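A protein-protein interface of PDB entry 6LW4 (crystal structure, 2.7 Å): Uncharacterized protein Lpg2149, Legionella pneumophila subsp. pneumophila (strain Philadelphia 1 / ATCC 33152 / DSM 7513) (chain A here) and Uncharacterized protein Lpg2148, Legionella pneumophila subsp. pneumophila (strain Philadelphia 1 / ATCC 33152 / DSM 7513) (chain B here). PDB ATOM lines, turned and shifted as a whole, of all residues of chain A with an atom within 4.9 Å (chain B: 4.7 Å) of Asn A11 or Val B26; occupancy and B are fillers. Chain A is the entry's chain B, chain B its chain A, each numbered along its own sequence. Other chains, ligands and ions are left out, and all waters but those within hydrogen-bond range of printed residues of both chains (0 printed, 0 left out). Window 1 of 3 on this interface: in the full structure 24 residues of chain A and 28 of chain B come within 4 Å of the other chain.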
ATOM      1  N   TYR A   7      26.626  -4.586 -11.841  1.00  0.00           N
ATOM      2  CA  TYR A   7      26.002  -4.393 -10.536  1.00  0.00           C
ATOM      3  C   TYR A   7      27.043  -4.497  -9.422  1.00  0.00           C
ATOM      4  O   TYR A   7      27.114  -3.647  -8.518  1.00  0.00           O
ATOM      5  CB  TYR A   7      24.894  -5.434 -10.381  1.00  0.00           C
ATOM      6  CG  TYR A   7      24.276  -5.578  -9.013  1.00  0.00           C
ATOM      7  CD1 TYR A   7      23.303  -4.691  -8.571  1.00  0.00           C
ATOM      8  CD2 TYR A   7      24.632  -6.629  -8.182  1.00  0.00           C
ATOM      9  CE1 TYR A   7      22.721  -4.836  -7.329  1.00  0.00           C
ATOM     10  CE2 TYR A   7      24.057  -6.782  -6.940  1.00  0.00           C
ATOM     11  CZ  TYR A   7      23.103  -5.884  -6.518  1.00  0.00           C
ATOM     12  OH  TYR A   7      22.530  -6.033  -5.277  1.00  0.00           O
ATOM     13  N   GLN A   8      27.879  -5.532  -9.491  1.00  0.00           N
ATOM     14  CA  GLN A   8      28.989  -5.669  -8.560  1.00  0.00           C
ATOM     15  C   GLN A   8      29.942  -4.486  -8.660  1.00  0.00           C
ATOM     16  O   GLN A   8      30.416  -3.979  -7.639  1.00  0.00           O
ATOM     17  CB  GLN A   8      29.723  -6.985  -8.831  1.00  0.00           C
ATOM     18  CG  GLN A   8      31.042  -7.137  -8.101  1.00  0.00           C
ATOM     19  CD  GLN A   8      31.689  -8.482  -8.359  1.00  0.00           C
ATOM     20  OE1 GLN A   8      32.449  -8.649  -9.317  1.00  0.00           O
ATOM     21  NE2 GLN A   8      31.391  -9.453  -7.504  1.00  0.00           N
ATOM     22  N   LYS A   9      30.235  -4.033  -9.883  1.00  0.00           N
ATOM     23  CA  LYS A   9      31.156  -2.914 -10.063  1.00  0.00           C
ATOM     24  C   LYS A   9      30.623  -1.652  -9.398  1.00  0.00           C
ATOM     25  O   LYS A   9      31.354  -0.957  -8.683  1.00  0.00           O
ATOM     26  CB  LYS A   9      31.409  -2.669 -11.552  1.00  0.00           C
ATOM     27  CG  LYS A   9      32.138  -1.363 -11.852  1.00  0.00           C
ATOM     28  CD  LYS A   9      32.358  -1.177 -13.348  1.00  0.00           C
ATOM     29  CE  LYS A   9      33.288  -0.005 -13.635  1.00  0.00           C
ATOM     30  NZ  LYS A   9      33.905  -0.099 -14.991  1.00  0.00           N
ATOM     31  N   LYS A  10      29.349  -1.333  -9.631  1.00  0.00           N
ATOM     32  CA  LYS A  10      28.788  -0.121  -9.045  1.00  0.00           C
ATOM     33  C   LYS A  10      28.750  -0.212  -7.523  1.00  0.00           C
ATOM     34  O   LYS A  10      29.031   0.775  -6.830  1.00  0.00           O
ATOM     35  CB  LYS A  10      27.396   0.162  -9.617  1.00  0.00           C
ATOM     36  CG  LYS A  10      26.331  -0.866  -9.264  1.00  0.00           C
ATOM     37  CD  LYS A  10      25.148  -0.250  -8.532  1.00  0.00           C
ATOM     38  CE  LYS A  10      24.380  -1.309  -7.762  1.00  0.00           C
ATOM     39  NZ  LYS A  10      23.349  -0.708  -6.878  1.00  0.00           N
ATOM     40  N   ASN A  11      28.443  -1.395  -6.977  1.00  0.00           N
ATOM     41  CA  ASN A  11      28.432  -1.513  -5.521  1.00  0.00           C
ATOM     42  C   ASN A  11      29.840  -1.424  -4.937  1.00  0.00           C
ATOM     43  O   ASN A  11      30.039  -0.819  -3.875  1.00  0.00           O
ATOM     44  CB  ASN A  11      27.739  -2.805  -5.101  1.00  0.00           C
ATOM     45  CG  ASN A  11      26.237  -2.643  -4.996  1.00  0.00           C
ATOM     46  OD1 ASN A  11      25.729  -1.522  -4.970  1.00  0.00           O
ATOM     47  ND2 ASN A  11      25.516  -3.757  -4.928  1.00  0.00           N
ATOM     48  N   VAL A  12      30.833  -2.001  -5.621  1.00  0.00           N
ATOM     49  CA  VAL A  12      32.217  -1.896  -5.160  1.00  0.00           C
ATOM     50  C   VAL A  12      32.673  -0.445  -5.185  1.00  0.00           C
ATOM     51  O   VAL A  12      33.315   0.037  -4.243  1.00  0.00           O
ATOM     52  CB  VAL A  12      33.139  -2.788  -6.013  1.00  0.00           C
ATOM     53  CG1 VAL A  12      34.600  -2.469  -5.732  1.00  0.00           C
ATOM     54  CG2 VAL A  12      32.860  -4.258  -5.750  1.00  0.00           C
ATOM     55  N   MET A  13      32.351   0.274  -6.263  1.00  0.00           N
ATOM     56  CA  MET A  13      32.736   1.677  -6.352  1.00  0.00           C
ATOM     57  C   MET A  13      32.045   2.509  -5.281  1.00  0.00           C
ATOM     58  O   MET A  13      32.653   3.427  -4.720  1.00  0.00           O
ATOM     59  CB  MET A  13      32.426   2.225  -7.745  1.00  0.00           C
ATOM     60  CG  MET A  13      33.376   1.740  -8.825  1.00  0.00           C
ATOM     61  SD  MET A  13      33.304   2.752 -10.314  1.00  0.00           S
ATOM     62  CE  MET A  13      31.563   2.661 -10.718  1.00  0.00           C
ATOM     63  N   ARG A  14      30.782   2.199  -4.973  1.00  0.00           N
ATOM     64  CA  ARG A  14      30.088   2.925  -3.914  1.00  0.00           C
ATOM     65  C   ARG A  14      30.735   2.677  -2.557  1.00  0.00           C
ATOM     66  O   ARG A  14      30.908   3.612  -1.763  1.00  0.00           O
ATOM     67  CB  ARG A  14      28.614   2.526  -3.880  1.00  0.00           C
ATOM     68  CG  ARG A  14      27.793   3.311  -2.874  1.00  0.00           C
ATOM     69  CD  ARG A  14      27.654   4.763  -3.307  1.00  0.00           C
ATOM     70  NE  ARG A  14      28.544   5.654  -2.566  1.00  0.00           N
ATOM     71  CZ  ARG A  14      28.198   6.855  -2.112  1.00  0.00           C
ATOM     72  NH1 ARG A  14      26.972   7.319  -2.317  1.00  0.00           N
ATOM     73  NH2 ARG A  14      29.080   7.590  -1.448  1.00  0.00           N
ATOM     74  N   LEU A  15      31.086   1.423  -2.267  1.00  0.00           N
ATOM     75  CA  LEU A  15      31.776   1.123  -1.015  1.00  0.00           C
ATOM     76  C   LEU A  15      33.113   1.851  -0.943  1.00  0.00           C
ATOM     77  O   LEU A  15      33.491   2.382   0.112  1.00  0.00           O
ATOM     78  CB  LEU A  15      31.962  -0.388  -0.879  1.00  0.00           C
ATOM     79  CG  LEU A  15      32.564  -0.941   0.409  1.00  0.00           C
ATOM     80  CD1 LEU A  15      31.668  -0.634   1.593  1.00  0.00           C
ATOM     81  CD2 LEU A  15      32.773  -2.441   0.273  1.00  0.00           C
ATOM     82  N   THR B  24      24.750  -7.716  -2.247  1.00  0.00           N
ATOM     83  CA  THR B  24      25.334  -6.557  -2.909  1.00  0.00           C
ATOM     84  C   THR B  24      26.259  -6.956  -4.046  1.00  0.00           C
ATOM     85  O   THR B  24      26.510  -6.141  -4.936  1.00  0.00           O
ATOM     86  CB  THR B  24      26.100  -5.692  -1.909  1.00  0.00           C
ATOM     87  OG1 THR B  24      27.338  -6.333  -1.585  1.00  0.00           O
ATOM     88  CG2 THR B  24      25.279  -5.483  -0.648  1.00  0.00           C
ATOM     89  N   GLY B  25      26.744  -8.197  -4.051  1.00  0.00           N
ATOM     90  CA  GLY B  25      27.718  -8.636  -5.024  1.00  0.00           C
ATOM     91  C   GLY B  25      29.147  -8.281  -4.689  1.00  0.00           C
ATOM     92  O   GLY B  25      30.059  -8.684  -5.424  1.00  0.00           O
ATOM     93  N   VAL B  26      29.376  -7.542  -3.608  1.00  0.00           N
ATOM     94  CA  VAL B  26      30.720  -7.147  -3.197  1.00  0.00           C
ATOM     95  C   VAL B  26      31.493  -8.378  -2.739  1.00  0.00           C
ATOM     96  O   VAL B  26      31.076  -9.048  -1.783  1.00  0.00           O
ATOM     97  CB  VAL B  26      30.674  -6.088  -2.085  1.00  0.00           C
ATOM     98  CG1 VAL B  26      32.073  -5.827  -1.547  1.00  0.00           C
ATOM     99  CG2 VAL B  26      30.038  -4.808  -2.598  1.00  0.00           C
ATOM    100  N   PRO B  27      32.610  -8.713  -3.387  1.00  0.00           N
ATOM    101  CA  PRO B  27      33.405  -9.865  -2.953  1.00  0.00           C
ATOM    102  C   PRO B  27      33.889  -9.703  -1.523  1.00  0.00           C
ATOM    103  O   PRO B  27      34.056  -8.589  -1.024  1.00  0.00           O
ATOM    104  CB  PRO B  27      34.578  -9.878  -3.939  1.00  0.00           C
ATOM    105  CG  PRO B  27      34.059  -9.166  -5.144  1.00  0.00           C
ATOM    106  CD  PRO B  27      33.151  -8.098  -4.611  1.00  0.00           C
ATOM    107  N   ALA B  28      34.109 -10.841  -0.860  1.00  0.00           N
ATOM    108  CA  ALA B  28      34.494 -10.806   0.546  1.00  0.00           C
ATOM    109  C   ALA B  28      35.853 -10.148   0.724  1.00  0.00           C
ATOM    110  O   ALA B  28      36.068  -9.407   1.690  1.00  0.00           O
ATOM    111  CB  ALA B  28      34.490 -12.218   1.126  1.00  0.00           C
ATOM    112  N   VAL B  30      37.258  -7.832  -1.196  1.00  0.00           N
ATOM    113  CA  VAL B  30      37.060  -6.393  -1.379  1.00  0.00           C
ATOM    114  C   VAL B  30      36.553  -5.763  -0.087  1.00  0.00           C
ATOM    115  O   VAL B  30      37.065  -4.731   0.379  1.00  0.00           O
ATOM    116  CB  VAL B  30      36.082  -6.139  -2.541  1.00  0.00           C
ATOM    117  CG1 VAL B  30      35.676  -4.679  -2.593  1.00  0.00           C
ATOM    118  CG2 VAL B  30      36.687  -6.586  -3.855  1.00  0.00           C
ATOM    119  N   LEU B  31      35.517  -6.375   0.494  1.00  0.00           N
ATOM    120  CA  LEU B  31      34.940  -5.881   1.738  1.00  0.00           C
ATOM    121  C   LEU B  31      35.980  -5.839   2.850  1.00  0.00           C
ATOM    122  O   LEU B  31      36.081  -4.843   3.578  1.00  0.00           O
ATOM    123  CB  LEU B  31      33.758  -6.763   2.135  1.00  0.00           C
ATOM    124  CG  LEU B  31      32.944  -6.366   3.364  1.00  0.00           C
ATOM    125  CD1 LEU B  31      32.291  -5.011   3.149  1.00  0.00           C
ATOM    126  CD2 LEU B  31      31.901  -7.427   3.662  1.00  0.00           C
ATOM    127  N   ASP B  77      19.984  -0.706  -5.134  1.00  0.00           N
ATOM    128  CA  ASP B  77      20.194  -2.120  -5.420  1.00  0.00           C
ATOM    129  C   ASP B  77      18.890  -2.799  -5.820  1.00  0.00           C
ATOM    130  O   ASP B  77      18.873  -3.626  -6.736  1.00  0.00           O
ATOM    131  CB  ASP B  77      20.811  -2.823  -4.211  1.00  0.00           C
ATOM    132  CG  ASP B  77      22.186  -2.286  -3.856  1.00  0.00           C
ATOM    133  OD1 ASP B  77      22.785  -1.576  -4.691  1.00  0.00           O
ATOM    134  OD2 ASP B  77      22.667  -2.577  -2.737  1.00  0.00           O
ATOM    135  N   PHE B 349      26.567 -16.108  -8.395  1.00  0.00           N
ATOM    136  CA  PHE B 349      27.656 -15.513  -7.622  1.00  0.00           C
ATOM    137  C   PHE B 349      27.699 -16.089  -6.210  1.00  0.00           C
ATOM    138  O   PHE B 349      28.761 -16.478  -5.711  1.00  0.00           O
ATOM    139  CB  PHE B 349      27.506 -13.992  -7.570  1.00  0.00           C
ATOM    140  CG  PHE B 349      28.328 -13.333  -6.483  1.00  0.00           C
ATOM    141  CD1 PHE B 349      29.694 -13.152  -6.640  1.00  0.00           C
ATOM    142  CD2 PHE B 349      27.728 -12.883  -5.310  1.00  0.00           C
ATOM    143  CE1 PHE B 349      30.449 -12.546  -5.651  1.00  0.00           C
ATOM    144  CE2 PHE B 349      28.479 -12.277  -4.314  1.00  0.00           C
ATOM    145  CZ  PHE B 349      29.842 -12.109  -4.486  1.00  0.00           C
ATOM    146  N   TYR B 365      31.742 -16.582   3.217  1.00  0.00           N
ATOM    147  CA  TYR B 365      31.909 -15.160   2.928  1.00  0.00           C
ATOM    148  C   TYR B 365      32.500 -14.420   4.124  1.00  0.00           C
ATOM    149  O   TYR B 365      33.432 -13.619   3.979  1.00  0.00           O
ATOM    150  CB  TYR B 365      30.561 -14.552   2.532  1.00  0.00           C
ATOM    151  CG  TYR B 365      30.618 -13.102   2.095  1.00  0.00           C
ATOM    152  CD1 TYR B 365      30.803 -12.767   0.758  1.00  0.00           C
ATOM    153  CD2 TYR B 365      30.466 -12.069   3.015  1.00  0.00           C
ATOM    154  CE1 TYR B 365      30.848 -11.446   0.351  1.00  0.00           C
ATOM    155  CE2 TYR B 365      30.511 -10.740   2.616  1.00  0.00           C
ATOM    156  CZ  TYR B 365      30.701 -10.440   1.283  1.00  0.00           C
ATOM    157  OH  TYR B 365      30.745  -9.130   0.876  1.00  0.00           O
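Among the printed residues, pairs that only touch across the chains: Tyr A7 with Thr B24 (3.2 Å), Gln A8 with Pro B27 (3.6 Å), Gln A8 with Phe B349 (3.7 Å), Tyr A7 with Asp B77 (3.8 Å), Leu A15 with Leu B31 (3.9 Å), Leu A15 with Val B26 (3.9 Å), Asn A11 with Val B26 (3.9 Å) and Val A12 with Val B30 (3.99 Å).
The side-chain hydroxyl (OG1) of Thr B24 is in hydrogen-bond range of the backbone NH (N) of Val B26 (3.1 Å). The side-chain hydroxyl of Tyr B365 sits at hydrogen-bond distance from the backbone carbonyl oxygen of Val B26 (2.7 Å). NZ of Lys A10 lies close to OD1 of Asn A11 (3.2 Å).
Of the printed residues of chain B, Asn A11 touches Thr B24 (2.6 Å), Val B26 (3.9 Å) and Asp B77 (3.0 Å). Val B26 touches just these residues of chain A: Asn A11 and Leu A15. Of the printed residues of chain A, Val B30 touches Val A12. Of the printed residues of chain A, Leu B31 touches Leu A15 (3.9 Å). Printed residues of chain A within 4 Å of Pro B27: Gln A8 (3.6 Å). Of the printed residues of chain B, Lys A10 touches Asp B77. The nearest printed residue of chain B that does not touch Asn A11 is Gly B25 (4.7 Å). The nearest residue of chain A that does not touch Val B26 is Val A12 (4.2 Å).
Of the 9 printed residues of chain A, 6 touch a printed residue of chain B. Hydrophobic or aromatic side chains of chain A that line the printed part of chain B: Tyr A7, Val A12 and Leu A15. Of the 10 printed residues of chain B, 8 touch a printed residue of chain A. Among the printed residues, Asp or Glu carboxylates within 4 Å of a Lys or Arg side-chain nitrogen of the other chain: Lys A10 with Asp B77 (2.4 Å).
The backbone carbonyl oxygen of Thr B24 lies within hydrogen-bond range of the side-chain amide nitrogen of Asn A11, at 2.6 Å. NE2 of Gln A8 is in hydrogen-bond range of O of Gly B25 (2.6 Å). The side-chain carboxylate (OD1) of Asp B77 lies within salt-bridge range of the side-chain amino group (NZ) of Lys A10 (2.4 Å). OD1 of Asp B77 sits close to OD1 of Asn A11 (3.0 Å).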
